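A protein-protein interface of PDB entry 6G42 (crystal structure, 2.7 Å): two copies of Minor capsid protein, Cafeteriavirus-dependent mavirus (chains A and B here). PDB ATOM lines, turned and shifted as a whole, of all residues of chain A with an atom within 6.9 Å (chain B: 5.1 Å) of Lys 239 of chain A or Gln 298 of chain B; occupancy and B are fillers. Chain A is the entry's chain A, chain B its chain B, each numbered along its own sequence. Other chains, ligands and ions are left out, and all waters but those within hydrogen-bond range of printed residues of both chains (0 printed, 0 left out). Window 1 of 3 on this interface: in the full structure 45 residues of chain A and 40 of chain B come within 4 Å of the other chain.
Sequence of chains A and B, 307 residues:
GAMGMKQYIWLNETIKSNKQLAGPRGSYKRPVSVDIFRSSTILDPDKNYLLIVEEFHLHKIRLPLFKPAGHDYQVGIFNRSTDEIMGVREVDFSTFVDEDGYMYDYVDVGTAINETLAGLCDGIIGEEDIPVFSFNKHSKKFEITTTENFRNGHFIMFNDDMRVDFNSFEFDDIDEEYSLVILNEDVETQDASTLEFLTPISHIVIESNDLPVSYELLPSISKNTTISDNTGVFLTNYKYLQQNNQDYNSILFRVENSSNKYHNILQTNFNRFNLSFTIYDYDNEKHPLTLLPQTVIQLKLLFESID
OG of Ser 202 of chain A sits at hydrogen-bond distance from NE2 of Gln 298 of chain B (3.1 Å).
The side-chain carboxylate (OE2) of Glu 55 of chain B lies within hydrogen-bond range of the side-chain amide nitrogen (ND2) of Asn 237 of chain A, 2.8 Å away.
NZ of Lys 239 of chain A sits at hydrogen-bond distance from OE1 of Gln 298 of chain B, at 3.1 Å.
NE2 of His 57 of chain B lies within hydrogen-bond range of OH of Tyr 282 of chain A.
ND1 of His 203 of chain A is in hydrogen-bond range of OG of Ser 202 of chain A (2.7 Å).
OG of Ser 202 of chain A is in hydrogen-bond range of NZ of Lys 239 of chain A (3.0 Å).
The backbone carbonyl oxygen (O) of Ser 202 of chain A lies within hydrogen-bond range of the backbone NH (N) of Tyr 240 of chain A (3.1 Å).
The backbone NH (N) of Ser 202 of chain A lies within hydrogen-bond range of the backbone carbonyl oxygen (O) of Tyr 280 of chain A (2.9 Å).
The backbone carbonyl oxygen (O) of Glu 55 of chain B sits at hydrogen-bond distance from the backbone NH (N) of Lys 300 of chain B, at 2.8 Å.
The backbone carbonyl oxygen (O) of Gln 298 of chain B lies within hydrogen-bond range of the backbone NH (N) of His 57 of chain B (3.0 Å).
Among the printed residues, pairs that only touch across the chains: Lys 239 of chain A with His 57 of chain B, Lys 239 of chain A with Leu 252 of chain B, Tyr 282 of chain A with Val 296 of chain B, Lys 239 of chain A with Arg 254 of chain B and His 203 of chain A with Gln 298 of chain B.
Lys 239 of chain A touches just these residues of chain B: His 57, Leu 252, Arg 254 and Gln 298.
Printed residues of chain A within 4 Å of Gln 298 of chain B: Ser 202, His 203 and Lys 239.
Printed residues of chain B within 4 Å of Tyr 282 of chain A: His 57 and Val 296.
Printed residues of chain A within 4 Å of Val 296 of chain B: Tyr 282.
Glu 13 of chain B touches none of the printed residues of chain A.
Lys 300 of chain B touches none of the printed residues of chain A.
The nearest residue of chain B that does not touch Lys 239 of chain A is Glu 55 of chain B (4.6 Å).
Hydrophobic or aromatic side chains of chain B within 4 Å of the printed part of chain A: His 57, Leu 252 and Val 296.
Along chain A the printed residues that touch a printed residue of chain B span positions 202 to 282.
Among the printed residues, 9 pairs touch across the chains.
Among the printed residues, no Asp or Glu carboxylate lies within 4 Å of a Lys or Arg side-chain nitrogen of the other chain.
No position is printed for both chains.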
ATOM      1  N   ILE A 201      32.231 -14.748 -14.438  1.00  0.00           N
ATOM      2  CA  ILE A 201      31.647 -13.982 -15.541  1.00  0.00           C
ATOM      3  C   ILE A 201      30.285 -13.421 -15.128  1.00  0.00           C
ATOM      4  O   ILE A 201      29.355 -14.182 -14.859  1.00  0.00           O
ATOM      5  CB  ILE A 201      31.435 -14.852 -16.807  1.00  0.00           C
ATOM      6  CG1 ILE A 201      32.691 -15.637 -17.209  1.00  0.00           C
ATOM      7  CG2 ILE A 201      30.972 -13.999 -17.983  1.00  0.00           C
ATOM      8  CD1 ILE A 201      33.922 -14.805 -17.462  1.00  0.00           C
ATOM      9  N   SER A 202      30.164 -12.097 -15.097  1.00  0.00           N
ATOM     10  CA  SER A 202      28.879 -11.455 -14.814  1.00  0.00           C
ATOM     11  C   SER A 202      28.106 -11.180 -16.105  1.00  0.00           C
ATOM     12  O   SER A 202      27.082 -11.819 -16.351  1.00  0.00           O
ATOM     13  CB  SER A 202      29.057 -10.178 -13.988  1.00  0.00           C
ATOM     14  OG  SER A 202      27.804  -9.554 -13.774  1.00  0.00           O
ATOM     15  N   HIS A 203      28.582 -10.252 -16.926  1.00  0.00           N
ATOM     16  CA  HIS A 203      27.918  -9.979 -18.197  1.00  0.00           C
ATOM     17  C   HIS A 203      28.886  -9.697 -19.335  1.00  0.00           C
ATOM     18  O   HIS A 203      30.058  -9.378 -19.118  1.00  0.00           O
ATOM     19  CB  HIS A 203      26.887  -8.852 -18.059  1.00  0.00           C
ATOM     20  CG  HIS A 203      27.333  -7.701 -17.214  1.00  0.00           C
ATOM     21  ND1 HIS A 203      27.466  -7.787 -15.845  1.00  0.00           N
ATOM     22  CD2 HIS A 203      27.631  -6.423 -17.540  1.00  0.00           C
ATOM     23  CE1 HIS A 203      27.848  -6.616 -15.368  1.00  0.00           C
ATOM     24  NE2 HIS A 203      27.955  -5.771 -16.377  1.00  0.00           N
ATOM     25  N   ILE A 204      28.357  -9.825 -20.548  1.00  0.00           N
ATOM     26  CA  ILE A 204      29.092  -9.559 -21.785  1.00  0.00           C
ATOM     27  C   ILE A 204      28.447  -8.308 -22.380  1.00  0.00           C
ATOM     28  O   ILE A 204      27.220  -8.205 -22.439  1.00  0.00           O
ATOM     29  CB  ILE A 204      29.030 -10.733 -22.782  1.00  0.00           C
ATOM     30  CG1 ILE A 204      29.620 -11.987 -22.136  1.00  0.00           C
ATOM     31  CG2 ILE A 204      29.803 -10.387 -24.057  1.00  0.00           C
ATOM     32  CD1 ILE A 204      29.515 -13.240 -22.970  1.00  0.00           C
ATOM     33  N   ASN A 237      23.736  -5.420 -23.007  1.00  0.00           N
ATOM     34  CA  ASN A 237      24.109  -5.901 -21.684  1.00  0.00           C
ATOM     35  C   ASN A 237      23.560  -7.326 -21.500  1.00  0.00           C
ATOM     36  O   ASN A 237      22.412  -7.516 -21.080  1.00  0.00           O
ATOM     37  CB  ASN A 237      23.522  -4.924 -20.655  1.00  0.00           C
ATOM     38  CG  ASN A 237      24.182  -5.013 -19.303  1.00  0.00           C
ATOM     39  OD1 ASN A 237      25.394  -4.859 -19.192  1.00  0.00           O
ATOM     40  ND2 ASN A 237      23.381  -5.217 -18.255  1.00  0.00           N
ATOM     41  N   TYR A 238      24.382  -8.318 -21.832  1.00  0.00           N
ATOM     42  CA  TYR A 238      23.970  -9.726 -21.798  1.00  0.00           C
ATOM     43  C   TYR A 238      24.412 -10.405 -20.501  1.00  0.00           C
ATOM     44  O   TYR A 238      25.604 -10.581 -20.280  1.00  0.00           O
ATOM     45  CB  TYR A 238      24.550 -10.479 -23.007  1.00  0.00           C
ATOM     46  CG  TYR A 238      24.194 -11.960 -23.080  1.00  0.00           C
ATOM     47  CD1 TYR A 238      23.031 -12.389 -23.718  1.00  0.00           C
ATOM     48  CD2 TYR A 238      25.033 -12.934 -22.523  1.00  0.00           C
ATOM     49  CE1 TYR A 238      22.707 -13.739 -23.791  1.00  0.00           C
ATOM     50  CE2 TYR A 238      24.716 -14.286 -22.593  1.00  0.00           C
ATOM     51  CZ  TYR A 238      23.554 -14.683 -23.227  1.00  0.00           C
ATOM     52  OH  TYR A 238      23.230 -16.020 -23.303  1.00  0.00           O
ATOM     53  N   LYS A 239      23.449 -10.808 -19.673  1.00  0.00           N
ATOM     54  CA  LYS A 239      23.725 -11.566 -18.456  1.00  0.00           C
ATOM     55  C   LYS A 239      24.138 -13.004 -18.775  1.00  0.00           C
ATOM     56  O   LYS A 239      23.403 -13.722 -19.451  1.00  0.00           O
ATOM     57  CB  LYS A 239      22.495 -11.590 -17.541  1.00  0.00           C
ATOM     58  CG  LYS A 239      22.739 -12.159 -16.143  1.00  0.00           C
ATOM     59  CD  LYS A 239      23.860 -11.403 -15.459  1.00  0.00           C
ATOM     60  CE  LYS A 239      24.006 -11.716 -13.992  1.00  0.00           C
ATOM     61  NZ  LYS A 239      25.089 -10.835 -13.474  1.00  0.00           N
ATOM     62  N   TYR A 240      25.300 -13.417 -18.269  1.00  0.00           N
ATOM     63  CA  TYR A 240      25.850 -14.746 -18.535  1.00  0.00           C
ATOM     64  C   TYR A 240      25.584 -15.719 -17.386  1.00  0.00           C
ATOM     65  O   TYR A 240      25.671 -15.351 -16.215  1.00  0.00           O
ATOM     66  CB  TYR A 240      27.350 -14.661 -18.784  1.00  0.00           C
ATOM     67  CG  TYR A 240      27.961 -15.997 -19.144  1.00  0.00           C
ATOM     68  CD1 TYR A 240      27.762 -16.558 -20.404  1.00  0.00           C
ATOM     69  CD2 TYR A 240      28.714 -16.711 -18.222  1.00  0.00           C
ATOM     70  CE1 TYR A 240      28.312 -17.785 -20.739  1.00  0.00           C
ATOM     71  CE2 TYR A 240      29.268 -17.938 -18.544  1.00  0.00           C
ATOM     72  CZ  TYR A 240      29.068 -18.471 -19.804  1.00  0.00           C
ATOM     73  OH  TYR A 240      29.606 -19.694 -20.139  1.00  0.00           O
ATOM     74  N   LEU A 241      25.276 -16.964 -17.732  1.00  0.00           N
ATOM     75  CA  LEU A 241      25.022 -18.000 -16.737  1.00  0.00           C
ATOM     76  C   LEU A 241      25.785 -19.256 -17.126  1.00  0.00           C
ATOM     77  O   LEU A 241      25.640 -19.750 -18.238  1.00  0.00           O
ATOM     78  CB  LEU A 241      23.517 -18.280 -16.614  1.00  0.00           C
ATOM     79  CG  LEU A 241      22.675 -17.119 -16.043  1.00  0.00           C
ATOM     80  CD1 LEU A 241      21.186 -17.352 -16.268  1.00  0.00           C
ATOM     81  CD2 LEU A 241      22.952 -16.858 -14.568  1.00  0.00           C
ATOM     82  N   TYR A 280      32.681  -8.473 -18.300  1.00  0.00           N
ATOM     83  CA  TYR A 280      32.741  -7.929 -16.943  1.00  0.00           C
ATOM     84  C   TYR A 280      32.603  -9.056 -15.928  1.00  0.00           C
ATOM     85  O   TYR A 280      31.687  -9.871 -16.030  1.00  0.00           O
ATOM     86  CB  TYR A 280      31.616  -6.912 -16.720  1.00  0.00           C
ATOM     87  CG  TYR A 280      31.920  -5.537 -17.258  1.00  0.00           C
ATOM     88  CD1 TYR A 280      31.696  -5.230 -18.598  1.00  0.00           C
ATOM     89  CD2 TYR A 280      32.437  -4.535 -16.427  1.00  0.00           C
ATOM     90  CE1 TYR A 280      31.977  -3.963 -19.101  1.00  0.00           C
ATOM     91  CE2 TYR A 280      32.722  -3.263 -16.920  1.00  0.00           C
ATOM     92  CZ  TYR A 280      32.492  -2.980 -18.257  1.00  0.00           C
ATOM     93  OH  TYR A 280      32.769  -1.731 -18.763  1.00  0.00           O
ATOM     94  N   ASP A 281      33.508  -9.089 -14.951  1.00  0.00           N
ATOM     95  CA  ASP A 281      33.433 -10.043 -13.842  1.00  0.00           C
ATOM     96  C   ASP A 281      32.653  -9.454 -12.653  1.00  0.00           C
ATOM     97  O   ASP A 281      32.401  -8.248 -12.595  1.00  0.00           O
ATOM     98  CB  ASP A 281      34.837 -10.473 -13.391  1.00  0.00           C
ATOM     99  CG  ASP A 281      35.607 -11.253 -14.464  1.00  0.00           C
ATOM    100  OD1 ASP A 281      35.068 -11.503 -15.563  1.00  0.00           O
ATOM    101  OD2 ASP A 281      36.774 -11.620 -14.203  1.00  0.00           O
ATOM    102  N   TYR A 282      32.292 -10.315 -11.703  1.00  0.00           N
ATOM    103  CA  TYR A 282      31.570  -9.907 -10.483  1.00  0.00           C
ATOM    104  C   TYR A 282      32.342  -8.936  -9.586  1.00  0.00           C
ATOM    105  O   TYR A 282      31.728  -8.178  -8.831  1.00  0.00           O
ATOM    106  CB  TYR A 282      31.135 -11.135  -9.671  1.00  0.00           C
ATOM    107  CG  TYR A 282      29.970 -11.846 -10.303  1.00  0.00           C
ATOM    108  CD1 TYR A 282      28.701 -11.267 -10.303  1.00  0.00           C
ATOM    109  CD2 TYR A 282      30.130 -13.071 -10.934  1.00  0.00           C
ATOM    110  CE1 TYR A 282      27.626 -11.898 -10.899  1.00  0.00           C
ATOM    111  CE2 TYR A 282      29.054 -13.710 -11.534  1.00  0.00           C
ATOM    112  CZ  TYR A 282      27.804 -13.118 -11.514  1.00  0.00           C
ATOM    113  OH  TYR A 282      26.735 -13.744 -12.102  1.00  0.00           O
ATOM    114  N   ASP A 283      33.673  -8.961  -9.680  1.00  0.00           N
ATOM    115  CA  ASP A 283      34.532  -7.927  -9.066  1.00  0.00           C
ATOM    116  C   ASP A 283      34.683  -6.656  -9.923  1.00  0.00           C
ATOM    117  O   ASP A 283      35.515  -5.798  -9.627  1.00  0.00           O
ATOM    118  CB  ASP A 283      35.909  -8.502  -8.681  1.00  0.00           C
ATOM    119  CG  ASP A 283      36.641  -9.150  -9.843  1.00  0.00           C
ATOM    120  OD1 ASP A 283      36.634  -8.600 -10.965  1.00  0.00           O
ATOM    121  OD2 ASP A 283      37.243 -10.227  -9.627  1.00  0.00           O
ATOM    122  N   ASN A 284      33.883  -6.553 -10.985  1.00  0.00           N
ATOM    123  CA  ASN A 284      33.850  -5.409 -11.902  1.00  0.00           C
ATOM    124  C   ASN A 284      35.117  -5.216 -12.760  1.00  0.00           C
ATOM    125  O   ASN A 284      35.257  -4.185 -13.422  1.00  0.00           O
ATOM    126  CB  ASN A 284      33.491  -4.119 -11.140  1.00  0.00           C
ATOM    127  CG  ASN A 284      32.474  -3.264 -11.882  1.00  0.00           C
ATOM    128  OD1 ASN A 284      32.624  -2.989 -13.072  1.00  0.00           O
ATOM    129  ND2 ASN A 284      31.431  -2.836 -11.178  1.00  0.00           N
ATOM    130  N   GLU B  13      24.034   0.739 -10.763  1.00  0.00           N
ATOM    131  CA  GLU B  13      24.582   0.748  -9.411  1.00  0.00           C
ATOM    132  C   GLU B  13      25.000  -0.646  -8.962  1.00  0.00           C
ATOM    133  O   GLU B  13      24.379  -1.636  -9.334  1.00  0.00           O
ATOM    134  CB  GLU B  13      23.568   1.328  -8.416  1.00  0.00           C
ATOM    135  CG  GLU B  13      23.654   2.835  -8.210  1.00  0.00           C
ATOM    136  CD  GLU B  13      25.024   3.326  -7.759  1.00  0.00           C
ATOM    137  OE1 GLU B  13      25.759   2.568  -7.084  1.00  0.00           O
ATOM    138  OE2 GLU B  13      25.361   4.484  -8.085  1.00  0.00           O
ATOM    139  N   THR B  14      26.052  -0.700  -8.149  1.00  0.00           N
ATOM    140  CA  THR B  14      26.579  -1.956  -7.614  1.00  0.00           C
ATOM    141  C   THR B  14      26.969  -1.823  -6.141  1.00  0.00           C
ATOM    142  O   THR B  14      27.303  -0.737  -5.673  1.00  0.00           O
ATOM    143  CB  THR B  14      27.804  -2.439  -8.411  1.00  0.00           C
ATOM    144  OG1 THR B  14      28.785  -1.400  -8.459  1.00  0.00           O
ATOM    145  CG2 THR B  14      27.415  -2.809  -9.833  1.00  0.00           C
ATOM    146  N   GLU B  55      16.682  -4.414 -14.503  1.00  0.00           N
ATOM    147  CA  GLU B  55      17.178  -5.626 -13.858  1.00  0.00           C
ATOM    148  C   GLU B  55      17.887  -5.366 -12.547  1.00  0.00           C
ATOM    149  O   GLU B  55      18.335  -4.253 -12.264  1.00  0.00           O
ATOM    150  CB  GLU B  55      18.094  -6.437 -14.790  1.00  0.00           C
ATOM    151  CG  GLU B  55      19.385  -5.784 -15.247  1.00  0.00           C
ATOM    152  CD  GLU B  55      20.173  -6.649 -16.245  1.00  0.00           C
ATOM    153  OE1 GLU B  55      20.009  -7.898 -16.262  1.00  0.00           O
ATOM    154  OE2 GLU B  55      20.987  -6.077 -17.013  1.00  0.00           O
ATOM    155  N   PHE B  56      17.935  -6.410 -11.731  1.00  0.00           N
ATOM    156  CA  PHE B  56      18.837  -6.470 -10.595  1.00  0.00           C
ATOM    157  C   PHE B  56      19.354  -7.886 -10.468  1.00  0.00           C
ATOM    158  O   PHE B  56      18.797  -8.813 -11.055  1.00  0.00           O
ATOM    159  CB  PHE B  56      18.166  -6.004  -9.288  1.00  0.00           C
ATOM    160  CG  PHE B  56      17.010  -6.864  -8.831  1.00  0.00           C
ATOM    161  CD1 PHE B  56      17.234  -8.081  -8.183  1.00  0.00           C
ATOM    162  CD2 PHE B  56      15.699  -6.436  -9.007  1.00  0.00           C
ATOM    163  CE1 PHE B  56      16.177  -8.865  -7.751  1.00  0.00           C
ATOM    164  CE2 PHE B  56      14.638  -7.216  -8.579  1.00  0.00           C
ATOM    165  CZ  PHE B  56      14.874  -8.432  -7.945  1.00  0.00           C
ATOM    166  N   HIS B  57      20.418  -8.039  -9.691  1.00  0.00           N
ATOM    167  CA  HIS B  57      21.009  -9.343  -9.434  1.00  0.00           C
ATOM    168  C   HIS B  57      21.493  -9.365  -8.000  1.00  0.00           C
ATOM    169  O   HIS B  57      22.432  -8.655  -7.658  1.00  0.00           O
ATOM    170  CB  HIS B  57      22.151  -9.612 -10.416  1.00  0.00           C
ATOM    171  CG  HIS B  57      22.685 -11.012 -10.377  1.00  0.00           C
ATOM    172  ND1 HIS B  57      21.903 -12.118 -10.119  1.00  0.00           N
ATOM    173  CD2 HIS B  57      23.931 -11.484 -10.595  1.00  0.00           C
ATOM    174  CE1 HIS B  57      22.649 -13.207 -10.171  1.00  0.00           C
ATOM    175  NE2 HIS B  57      23.885 -12.850 -10.460  1.00  0.00           N
ATOM    176  N   LEU B 252      18.277 -13.623  -9.925  1.00  0.00           N
ATOM    177  CA  LEU B 252      18.340 -12.780 -11.107  1.00  0.00           C
ATOM    178  C   LEU B 252      16.934 -12.363 -11.509  1.00  0.00           C
ATOM    179  O   LEU B 252      16.035 -13.195 -11.551  1.00  0.00           O
ATOM    180  CB  LEU B 252      19.008 -13.540 -12.250  1.00  0.00           C
ATOM    181  CG  LEU B 252      19.187 -12.808 -13.579  1.00  0.00           C
ATOM    182  CD1 LEU B 252      20.015 -11.541 -13.409  1.00  0.00           C
ATOM    183  CD2 LEU B 252      19.827 -13.747 -14.589  1.00  0.00           C
ATOM    184  N   ARG B 254      15.018 -10.018 -14.618  1.00  0.00           N
ATOM    185  CA  ARG B 254      15.085  -9.278 -15.870  1.00  0.00           C
ATOM    186  C   ARG B 254      13.673  -9.061 -16.386  1.00  0.00           C
ATOM    187  O   ARG B 254      12.862  -9.976 -16.394  1.00  0.00           O
ATOM    188  CB  ARG B 254      15.917 -10.036 -16.898  1.00  0.00           C
ATOM    189  CG  ARG B 254      17.410 -10.019 -16.604  1.00  0.00           C
ATOM    190  CD  ARG B 254      18.186 -10.863 -17.605  1.00  0.00           C
ATOM    191  NE  ARG B 254      17.956 -12.300 -17.417  1.00  0.00           N
ATOM    192  CZ  ARG B 254      18.493 -13.269 -18.161  1.00  0.00           C
ATOM    193  NH1 ARG B 254      19.315 -12.984 -19.171  1.00  0.00           N
ATOM    194  NH2 ARG B 254      18.215 -14.541 -17.886  1.00  0.00           N
ATOM    195  N   VAL B 296      27.535  -9.652  -3.941  1.00  0.00           N
ATOM    196  CA  VAL B 296      27.578  -8.614  -4.957  1.00  0.00           C
ATOM    197  C   VAL B 296      26.143  -8.341  -5.368  1.00  0.00           C
ATOM    198  O   VAL B 296      25.348  -9.265  -5.519  1.00  0.00           O
ATOM    199  CB  VAL B 296      28.395  -9.045  -6.188  1.00  0.00           C
ATOM    200  CG1 VAL B 296      28.373  -7.954  -7.263  1.00  0.00           C
ATOM    201  CG2 VAL B 296      29.826  -9.382  -5.777  1.00  0.00           C
ATOM    202  N   ILE B 297      25.814  -7.069  -5.538  1.00  0.00           N
ATOM    203  CA  ILE B 297      24.470  -6.669  -5.925  1.00  0.00           C
ATOM    204  C   ILE B 297      24.576  -5.739  -7.112  1.00  0.00           C
ATOM    205  O   ILE B 297      25.448  -4.878  -7.150  1.00  0.00           O
ATOM    206  CB  ILE B 297      23.712  -6.074  -4.718  1.00  0.00           C
ATOM    207  CG1 ILE B 297      23.253  -7.245  -3.836  1.00  0.00           C
ATOM    208  CG2 ILE B 297      22.514  -5.231  -5.155  1.00  0.00           C
ATOM    209  CD1 ILE B 297      22.806  -6.873  -2.466  1.00  0.00           C
ATOM    210  N   GLN B 298      23.718  -5.960  -8.103  1.00  0.00           N
ATOM    211  CA  GLN B 298      23.714  -5.163  -9.323  1.00  0.00           C
ATOM    212  C   GLN B 298      22.310  -4.644  -9.556  1.00  0.00           C
ATOM    213  O   GLN B 298      21.328  -5.227  -9.090  1.00  0.00           O
ATOM    214  CB  GLN B 298      24.200  -5.983 -10.515  1.00  0.00           C
ATOM    215  CG  GLN B 298      25.709  -6.179 -10.533  1.00  0.00           C
ATOM    216  CD  GLN B 298      26.196  -7.347 -11.393  1.00  0.00           C
ATOM    217  OE1 GLN B 298      25.409  -8.132 -11.928  1.00  0.00           O
ATOM    218  NE2 GLN B 298      27.512  -7.468 -11.517  1.00  0.00           N
ATOM    219  N   LEU B 299      22.229  -3.537 -10.280  1.00  0.00           N
ATOM    220  CA  LEU B 299      20.984  -2.808 -10.416  1.00  0.00           C
ATOM    221  C   LEU B 299      21.020  -1.928 -11.644  1.00  0.00           C
ATOM    222  O   LEU B 299      22.011  -1.253 -11.886  1.00  0.00           O
ATOM    223  CB  LEU B 299      20.778  -1.935  -9.182  1.00  0.00           C
ATOM    224  CG  LEU B 299      19.428  -1.229  -9.094  1.00  0.00           C
ATOM    225  CD1 LEU B 299      18.383  -2.123  -8.449  1.00  0.00           C
ATOM    226  CD2 LEU B 299      19.559   0.061  -8.320  1.00  0.00           C
ATOM    227  N   LYS B 300      19.925  -1.926 -12.398  1.00  0.00           N
ATOM    228  CA  LYS B 300      19.797  -1.076 -13.571  1.00  0.00           C
ATOM    229  C   LYS B 300      18.412  -0.472 -13.576  1.00  0.00           C
ATOM    230  O   LYS B 300      17.421  -1.194 -13.514  1.00  0.00           O
ATOM    231  CB  LYS B 300      20.040  -1.870 -14.850  1.00  0.00           C
ATOM    232  CG  LYS B 300      20.582  -1.024 -15.989  1.00  0.00           C
ATOM    233  CD  LYS B 300      21.043  -1.878 -17.164  1.00  0.00           C
ATOM    234  CE  LYS B 300      21.951  -1.093 -18.105  1.00  0.00           C
ATOM    235  NZ  LYS B 300      21.662  -1.382 -19.536  1.00  0.00           N
